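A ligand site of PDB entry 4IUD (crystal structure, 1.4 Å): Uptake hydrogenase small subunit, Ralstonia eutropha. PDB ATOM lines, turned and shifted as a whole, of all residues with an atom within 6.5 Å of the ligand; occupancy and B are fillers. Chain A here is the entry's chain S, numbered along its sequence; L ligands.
C of Arg 192 touches S2 of the ligand, at 3.8 Å. CB of Phe 196 touches S2 of the ligand, 3.9 Å away. Tyr 217 touches the ligand. CA of Gly 223 touches S4 of the ligand (3.9 Å). CD of Pro 224 touches S3 of the ligand, 3.9 Å away. Ile 243 touches the ligand (CD1 to S4, 3.8 Å). Hydrophobic or aromatic side chains within 4 Å of the ligand: His 187, Phe 196, Tyr 217, Pro 224 and Ile 243. Along chain A the residues within 4 Å of the ligand span positions 187 to 243. The nearest printed residue that does not touch the ligand is Ile 186 (4.2 Å).
The side-chain hydroxyl of Tyr 191 sits at hydrogen-bond distance from the guanidinium group of Arg 192, at 3.0 Å. The backbone NH of His 187 is in hydrogen-bond range of the backbone carbonyl oxygen of Gly 223 (3.3 Å). The guanidinium group of Arg 192 sits at hydrogen-bond distance from the backbone carbonyl oxygen of Ile 243 (3.0 Å). The side-chain sulfur (SG) of Cys 215 sits close to the backbone NH (N) of Tyr 217, 3.3 Å away. The backbone carbonyl oxygen (O) of Leu 216 sits at hydrogen-bond distance from the backbone NH (N) of Cys 221 (3.2 Å). NH1 of Arg 192 lies within hydrogen-bond range of O of Phe 214, 2.8 Å away. SG of Cys 190 sits close to N of Arg 192, 3.5 Å away. The side-chain sulfur of Cys 221 lies close to the backbone NH of Cys 249.
An iron atom (FE1) of the ligand is bound by a ring nitrogen (ND1) of His 187, at 2.0 Å. SG of Cys 190 is bound to FE3 of the ligand (2.3 Å). The side-chain sulfur (SG) of Cys 221 is bound to an iron atom (FE2) of the ligand (2.3 Å). A sulfur (S2) of the ligand lies close to the backbone NH (N) of Arg 193. SG of Cys 215 is bound to FE4 of the ligand, at 2.3 Å. S1 of the ligand sits close to N of Leu 216, 3.5 Å away.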
ATOM      1  N   ILE A 186     -28.637  19.362  18.847  1.00  0.00           N
ATOM      2  CA  ILE A 186     -28.524  20.394  19.896  1.00  0.00           C
ATOM      3  C   ILE A 186     -29.693  21.382  19.782  1.00  0.00           C
ATOM      4  O   ILE A 186     -30.322  21.739  20.780  1.00  0.00           O
ATOM      5  CB  ILE A 186     -27.187  21.177  19.779  1.00  0.00           C
ATOM      6  CG1 ILE A 186     -25.976  20.242  19.835  1.00  0.00           C
ATOM      7  CG2 ILE A 186     -27.064  22.198  20.897  1.00  0.00           C
ATOM      8  CD1 ILE A 186     -25.919  19.391  21.067  1.00  0.00           C
ATOM      9  N   HIS A 187     -29.975  21.773  18.548  1.00  0.00           N
ATOM     10  CA  HIS A 187     -30.981  22.787  18.198  1.00  0.00           C
ATOM     11  C   HIS A 187     -32.418  22.391  18.533  1.00  0.00           C
ATOM     12  O   HIS A 187     -33.270  23.261  18.668  1.00  0.00           O
ATOM     13  CB  HIS A 187     -30.822  23.065  16.696  1.00  0.00           C
ATOM     14  CG  HIS A 187     -31.649  24.193  16.152  1.00  0.00           C
ATOM     15  ND1 HIS A 187     -31.324  25.489  16.341  1.00  0.00           N
ATOM     16  CD2 HIS A 187     -32.774  24.187  15.327  1.00  0.00           C
ATOM     17  CE1 HIS A 187     -32.215  26.265  15.704  1.00  0.00           C
ATOM     18  NE2 HIS A 187     -33.095  25.475  15.085  1.00  0.00           N
ATOM     19  N   ASP A 188     -32.687  21.087  18.669  1.00  0.00           N
ATOM     20  CA  ASP A 188     -34.041  20.619  18.985  1.00  0.00           C
ATOM     21  C   ASP A 188     -34.566  21.217  20.288  1.00  0.00           C
ATOM     22  O   ASP A 188     -35.681  21.757  20.330  1.00  0.00           O
ATOM     23  CB  ASP A 188     -34.089  19.072  19.108  1.00  0.00           C
ATOM     24  CG  ASP A 188     -33.828  18.357  17.782  1.00  0.00           C
ATOM     25  OD1 ASP A 188     -33.902  18.999  16.709  1.00  0.00           O
ATOM     26  OD2 ASP A 188     -33.556  17.128  17.812  1.00  0.00           O
ATOM     27  N   CYS A 190     -32.415  23.235  22.486  1.00  0.00           N
ATOM     28  CA  CYS A 190     -31.604  24.376  22.929  1.00  0.00           C
ATOM     29  C   CYS A 190     -32.505  25.448  23.520  1.00  0.00           C
ATOM     30  O   CYS A 190     -33.483  25.857  22.885  1.00  0.00           O
ATOM     31  CB  CYS A 190     -30.812  24.953  21.771  1.00  0.00           C
ATOM     32  SG  CYS A 190     -29.775  26.346  22.239  1.00  0.00           S
ATOM     33  N   TYR A 191     -32.173  25.915  24.716  1.00  0.00           N
ATOM     34  CA  TYR A 191     -33.002  26.908  25.413  1.00  0.00           C
ATOM     35  C   TYR A 191     -33.065  28.263  24.672  1.00  0.00           C
ATOM     36  O   TYR A 191     -33.961  29.052  24.924  1.00  0.00           O
ATOM     37  CB  TYR A 191     -32.539  27.123  26.859  1.00  0.00           C
ATOM     38  CG  TYR A 191     -31.352  28.044  26.972  1.00  0.00           C
ATOM     39  CD1 TYR A 191     -30.067  27.606  26.676  1.00  0.00           C
ATOM     40  CD2 TYR A 191     -31.518  29.372  27.364  1.00  0.00           C
ATOM     41  CE1 TYR A 191     -28.990  28.451  26.767  1.00  0.00           C
ATOM     42  CE2 TYR A 191     -30.443  30.230  27.466  1.00  0.00           C
ATOM     43  CZ  TYR A 191     -29.167  29.762  27.160  1.00  0.00           C
ATOM     44  OH  TYR A 191     -28.097  30.598  27.243  1.00  0.00           O
ATOM     45  N   ARG A 192     -32.126  28.519  23.747  1.00  0.00           N
ATOM     46  CA  ARG A 192     -32.183  29.737  22.918  1.00  0.00           C
ATOM     47  C   ARG A 192     -33.082  29.592  21.675  1.00  0.00           C
ATOM     48  O   ARG A 192     -33.200  30.525  20.898  1.00  0.00           O
ATOM     49  CB  ARG A 192     -30.763  30.172  22.506  1.00  0.00           C
ATOM     50  CG  ARG A 192     -29.860  30.471  23.683  1.00  0.00           C
ATOM     51  CD  ARG A 192     -28.620  31.254  23.290  1.00  0.00           C
ATOM     52  NE  ARG A 192     -27.747  31.453  24.439  1.00  0.00           N
ATOM     53  CZ  ARG A 192     -26.864  32.448  24.586  1.00  0.00           C
ATOM     54  NH1 ARG A 192     -26.698  33.367  23.639  1.00  0.00           N
ATOM     55  NH2 ARG A 192     -26.133  32.505  25.686  1.00  0.00           N
ATOM     56  N   ARG A 193     -33.705  28.423  21.509  1.00  0.00           N
ATOM     57  CA  ARG A 193     -34.556  28.151  20.333  1.00  0.00           C
ATOM     58  C   ARG A 193     -35.695  29.171  20.113  1.00  0.00           C
ATOM     59  O   ARG A 193     -35.957  29.558  18.976  1.00  0.00           O
ATOM     60  CB  ARG A 193     -35.107  26.716  20.398  1.00  0.00           C
ATOM     61  CG  ARG A 193     -35.944  26.274  19.212  1.00  0.00           C
ATOM     62  CD  ARG A 193     -35.151  26.249  17.908  1.00  0.00           C
ATOM     63  NE  ARG A 193     -36.007  25.824  16.798  1.00  0.00           N
ATOM     64  CZ  ARG A 193     -36.275  24.555  16.476  1.00  0.00           C
ATOM     65  NH1 ARG A 193     -35.762  23.538  17.170  1.00  0.00           N
ATOM     66  NH2 ARG A 193     -37.073  24.298  15.443  1.00  0.00           N
ATOM     67  N   PRO A 194     -36.368  29.619  21.205  1.00  0.00           N
ATOM     68  CA  PRO A 194     -37.399  30.648  21.014  1.00  0.00           C
ATOM     69  C   PRO A 194     -36.865  31.920  20.354  1.00  0.00           C
ATOM     70  O   PRO A 194     -37.581  32.562  19.584  1.00  0.00           O
ATOM     71  CB  PRO A 194     -37.886  30.922  22.440  1.00  0.00           C
ATOM     72  CG  PRO A 194     -37.633  29.641  23.155  1.00  0.00           C
ATOM     73  CD  PRO A 194     -36.335  29.128  22.588  1.00  0.00           C
ATOM     74  N   HIS A 195     -35.612  32.273  20.626  1.00  0.00           N
ATOM     75  CA  HIS A 195     -34.992  33.414  19.953  1.00  0.00           C
ATOM     76  C   HIS A 195     -34.737  33.120  18.492  1.00  0.00           C
ATOM     77  O   HIS A 195     -35.003  33.958  17.629  1.00  0.00           O
ATOM     78  CB  HIS A 195     -33.716  33.857  20.673  1.00  0.00           C
ATOM     79  CG  HIS A 195     -33.955  34.434  22.040  1.00  0.00           C
ATOM     80  ND1 HIS A 195     -34.797  35.467  22.260  1.00  0.00           N
ATOM     81  CD2 HIS A 195     -33.429  34.089  23.288  1.00  0.00           C
ATOM     82  CE1 HIS A 195     -34.815  35.762  23.562  1.00  0.00           C
ATOM     83  NE2 HIS A 195     -33.982  34.928  24.198  1.00  0.00           N
ATOM     84  N   PHE A 196     -34.219  31.932  18.188  1.00  0.00           N
ATOM     85  CA  PHE A 196     -34.037  31.512  16.787  1.00  0.00           C
ATOM     86  C   PHE A 196     -35.351  31.606  16.014  1.00  0.00           C
ATOM     87  O   PHE A 196     -35.396  32.184  14.923  1.00  0.00           O
ATOM     88  CB  PHE A 196     -33.512  30.070  16.706  1.00  0.00           C
ATOM     89  CG  PHE A 196     -33.374  29.559  15.301  1.00  0.00           C
ATOM     90  CD1 PHE A 196     -32.181  29.744  14.588  1.00  0.00           C
ATOM     91  CD2 PHE A 196     -34.427  28.879  14.670  1.00  0.00           C
ATOM     92  CE1 PHE A 196     -32.055  29.271  13.288  1.00  0.00           C
ATOM     93  CE2 PHE A 196     -34.296  28.415  13.370  1.00  0.00           C
ATOM     94  CZ  PHE A 196     -33.108  28.604  12.678  1.00  0.00           C
ATOM     95  N   PHE A 201     -31.067  37.294  17.078  1.00  0.00           N
ATOM     96  CA  PHE A 201     -29.701  36.789  16.956  1.00  0.00           C
ATOM     97  C   PHE A 201     -28.641  37.735  17.494  1.00  0.00           C
ATOM     98  O   PHE A 201     -28.736  38.969  17.347  1.00  0.00           O
ATOM     99  CB  PHE A 201     -29.388  36.541  15.475  1.00  0.00           C
ATOM    100  CG  PHE A 201     -30.313  35.576  14.797  1.00  0.00           C
ATOM    101  CD1 PHE A 201     -30.231  34.219  15.054  1.00  0.00           C
ATOM    102  CD2 PHE A 201     -31.257  36.026  13.892  1.00  0.00           C
ATOM    103  CE1 PHE A 201     -31.078  33.328  14.424  1.00  0.00           C
ATOM    104  CE2 PHE A 201     -32.114  35.140  13.254  1.00  0.00           C
ATOM    105  CZ  PHE A 201     -32.024  33.791  13.520  1.00  0.00           C
ATOM    106  N   PHE A 214     -29.557  35.889  23.181  1.00  0.00           N
ATOM    107  CA  PHE A 214     -30.163  35.650  21.854  1.00  0.00           C
ATOM    108  C   PHE A 214     -29.428  34.512  21.120  1.00  0.00           C
ATOM    109  O   PHE A 214     -28.311  34.140  21.483  1.00  0.00           O
ATOM    110  CB  PHE A 214     -30.163  36.927  21.016  1.00  0.00           C
ATOM    111  CG  PHE A 214     -31.281  37.895  21.340  1.00  0.00           C
ATOM    112  CD1 PHE A 214     -31.977  37.834  22.561  1.00  0.00           C
ATOM    113  CD2 PHE A 214     -31.606  38.904  20.445  1.00  0.00           C
ATOM    114  CE1 PHE A 214     -32.994  38.752  22.832  1.00  0.00           C
ATOM    115  CE2 PHE A 214     -32.620  39.808  20.715  1.00  0.00           C
ATOM    116  CZ  PHE A 214     -33.307  39.729  21.923  1.00  0.00           C
ATOM    117  N   CYS A 215     -30.089  33.959  20.109  1.00  0.00           N
ATOM    118  CA  CYS A 215     -29.559  32.789  19.385  1.00  0.00           C
ATOM    119  C   CYS A 215     -28.199  33.091  18.745  1.00  0.00           C
ATOM    120  O   CYS A 215     -27.950  34.220  18.300  1.00  0.00           O
ATOM    121  CB  CYS A 215     -30.568  32.328  18.325  1.00  0.00           C
ATOM    122  SG  CYS A 215     -29.954  31.111  17.153  1.00  0.00           S
ATOM    123  N   LEU A 216     -27.337  32.083  18.705  1.00  0.00           N
ATOM    124  CA  LEU A 216     -25.951  32.222  18.237  1.00  0.00           C
ATOM    125  C   LEU A 216     -25.732  31.719  16.795  1.00  0.00           C
ATOM    126  O   LEU A 216     -24.601  31.600  16.348  1.00  0.00           O
ATOM    127  CB  LEU A 216     -25.024  31.484  19.195  1.00  0.00           C
ATOM    128  CG  LEU A 216     -24.969  32.059  20.615  1.00  0.00           C
ATOM    129  CD1 LEU A 216     -24.326  31.094  21.592  1.00  0.00           C
ATOM    130  CD2 LEU A 216     -24.239  33.395  20.602  1.00  0.00           C
ATOM    131  N   TYR A 217     -26.826  31.448  16.066  1.00  0.00           N
ATOM    132  CA  TYR A 217     -26.752  30.963  14.674  1.00  0.00           C
ATOM    133  C   TYR A 217     -25.870  31.845  13.796  1.00  0.00           C
ATOM    134  O   TYR A 217     -25.026  31.337  13.044  1.00  0.00           O
ATOM    135  CB  TYR A 217     -28.160  30.894  14.067  1.00  0.00           C
ATOM    136  CG  TYR A 217     -28.249  30.294  12.673  1.00  0.00           C
ATOM    137  CD1 TYR A 217     -28.439  28.922  12.494  1.00  0.00           C
ATOM    138  CD2 TYR A 217     -28.189  31.086  11.538  1.00  0.00           C
ATOM    139  CE1 TYR A 217     -28.542  28.365  11.238  1.00  0.00           C
ATOM    140  CE2 TYR A 217     -28.289  30.538  10.271  1.00  0.00           C
ATOM    141  CZ  TYR A 217     -28.469  29.173  10.121  1.00  0.00           C
ATOM    142  OH  TYR A 217     -28.580  28.621   8.867  1.00  0.00           O
ATOM    143  N   LYS A 218     -26.059  33.152  13.885  1.00  0.00           N
ATOM    144  CA  LYS A 218     -25.270  34.066  13.037  1.00  0.00           C
ATOM    145  C   LYS A 218     -23.821  34.262  13.488  1.00  0.00           C
ATOM    146  O   LYS A 218     -23.009  34.813  12.753  1.00  0.00           O
ATOM    147  CB  LYS A 218     -25.988  35.405  12.897  1.00  0.00           C
ATOM    148  CG  LYS A 218     -27.323  35.262  12.181  1.00  0.00           C
ATOM    149  CD  LYS A 218     -27.990  36.596  11.908  1.00  0.00           C
ATOM    150  CE  LYS A 218     -29.187  36.404  10.988  1.00  0.00           C
ATOM    151  NZ  LYS A 218     -29.896  37.670  10.711  1.00  0.00           N
ATOM    152  N   CYS A 221     -23.017  29.085  15.175  1.00  0.00           N
ATOM    153  CA  CYS A 221     -23.486  27.922  15.939  1.00  0.00           C
ATOM    154  C   CYS A 221     -23.871  26.765  15.011  1.00  0.00           C
ATOM    155  O   CYS A 221     -24.698  26.929  14.112  1.00  0.00           O
ATOM    156  CB  CYS A 221     -24.673  28.280  16.825  1.00  0.00           C
ATOM    157  SG  CYS A 221     -25.242  26.880  17.824  1.00  0.00           S
ATOM    158  N   LYS A 222     -23.259  25.598  15.230  1.00  0.00           N
ATOM    159  CA  LYS A 222     -23.535  24.422  14.413  1.00  0.00           C
ATOM    160  C   LYS A 222     -24.519  23.457  15.104  1.00  0.00           C
ATOM    161  O   LYS A 222     -24.668  22.308  14.681  1.00  0.00           O
ATOM    162  CB  LYS A 222     -22.223  23.720  14.039  1.00  0.00           C
ATOM    163  CG  LYS A 222     -21.251  24.603  13.245  1.00  0.00           C
ATOM    164  CD  LYS A 222     -21.928  25.293  12.051  1.00  0.00           C
ATOM    165  CE  LYS A 222     -20.946  25.987  11.114  1.00  0.00           C
ATOM    166  NZ  LYS A 222     -20.070  27.001  11.763  1.00  0.00           N
ATOM    167  N   GLY A 223     -25.218  23.949  16.122  1.00  0.00           N
ATOM    168  CA  GLY A 223     -26.238  23.166  16.807  1.00  0.00           C
ATOM    169  C   GLY A 223     -27.297  22.548  15.884  1.00  0.00           C
ATOM    170  O   GLY A 223     -27.733  21.419  16.132  1.00  0.00           O
ATOM    171  N   PRO A 224     -27.718  23.276  14.834  1.00  0.00           N
ATOM    172  CA  PRO A 224     -28.738  22.718  13.925  1.00  0.00           C
ATOM    173  C   PRO A 224     -28.342  21.437  13.162  1.00  0.00           C
ATOM    174  O   PRO A 224     -29.221  20.725  12.658  1.00  0.00           O
ATOM    175  CB  PRO A 224     -29.014  23.865  12.943  1.00  0.00           C
ATOM    176  CG  PRO A 224     -28.701  25.087  13.745  1.00  0.00           C
ATOM    177  CD  PRO A 224     -27.506  24.717  14.561  1.00  0.00           C
ATOM    178  N   PHE A 241     -23.562  24.424  29.139  1.00  0.00           N
ATOM    179  CA  PHE A 241     -23.065  23.858  27.894  1.00  0.00           C
ATOM    180  C   PHE A 241     -22.576  25.013  27.024  1.00  0.00           C
ATOM    181  O   PHE A 241     -22.796  26.184  27.380  1.00  0.00           O
ATOM    182  CB  PHE A 241     -24.104  22.923  27.209  1.00  0.00           C
ATOM    183  CG  PHE A 241     -25.285  23.611  26.566  1.00  0.00           C
ATOM    184  CD1 PHE A 241     -26.220  24.300  27.332  1.00  0.00           C
ATOM    185  CD2 PHE A 241     -25.523  23.469  25.199  1.00  0.00           C
ATOM    186  CE1 PHE A 241     -27.335  24.883  26.733  1.00  0.00           C
ATOM    187  CE2 PHE A 241     -26.637  24.052  24.600  1.00  0.00           C
ATOM    188  CZ  PHE A 241     -27.538  24.757  25.370  1.00  0.00           C
ATOM    189  N   ILE A 243     -23.370  26.738  24.424  1.00  0.00           N
ATOM    190  CA  ILE A 243     -24.326  27.793  24.076  1.00  0.00           C
ATOM    191  C   ILE A 243     -24.778  28.608  25.291  1.00  0.00           C
ATOM    192  O   ILE A 243     -24.841  29.843  25.230  1.00  0.00           O
ATOM    193  CB  ILE A 243     -25.533  27.203  23.316  1.00  0.00           C
ATOM    194  CG1 ILE A 243     -25.097  26.820  21.896  1.00  0.00           C
ATOM    195  CG2 ILE A 243     -26.702  28.184  23.273  1.00  0.00           C
ATOM    196  CD1 ILE A 243     -25.795  25.595  21.335  1.00  0.00           C
ATOM    197  N   GLY A 248     -21.210  29.546  20.260  1.00  0.00           N
ATOM    198  CA  GLY A 248     -21.921  28.597  19.437  1.00  0.00           C
ATOM    199  C   GLY A 248     -21.320  27.196  19.537  1.00  0.00           C
ATOM    200  O   GLY A 248     -20.134  27.032  19.822  1.00  0.00           O
ATOM    201  N   CYS A 249     -22.159  26.194  19.340  1.00  0.00           N
ATOM    202  CA  CYS A 249     -21.691  24.833  19.110  1.00  0.00           C
ATOM    203  C   CYS A 249     -20.730  24.870  17.918  1.00  0.00           C
ATOM    204  O   CYS A 249     -21.003  25.528  16.916  1.00  0.00           O
ATOM    205  CB  CYS A 249     -22.896  23.921  18.838  1.00  0.00           C
ATOM    206  SG  CYS A 249     -22.541  22.185  18.464  1.00  0.00           S
HETATM  207 FE1  LIG L   1     -30.038  26.493  17.520  1.00  0.00          FE
HETATM  208 FE2  LIG L   1     -27.471  27.312  18.198  1.00  0.00          FE
HETATM  209 FE3  LIG L   1     -29.436  27.144  20.119  1.00  0.00          FE
HETATM  210 FE4  LIG L   1     -29.546  29.106  18.197  1.00  0.00          FE
HETATM  211  S1  LIG L   1     -28.063  28.836  19.766  1.00  0.00           S
HETATM  212  S2  LIG L   1     -31.246  27.817  18.928  1.00  0.00           S
HETATM  213  S3  LIG L   1     -28.658  27.943  16.471  1.00  0.00           S
HETATM  214  S4  LIG L   1     -28.615  25.463  18.826  1.00  0.00           S
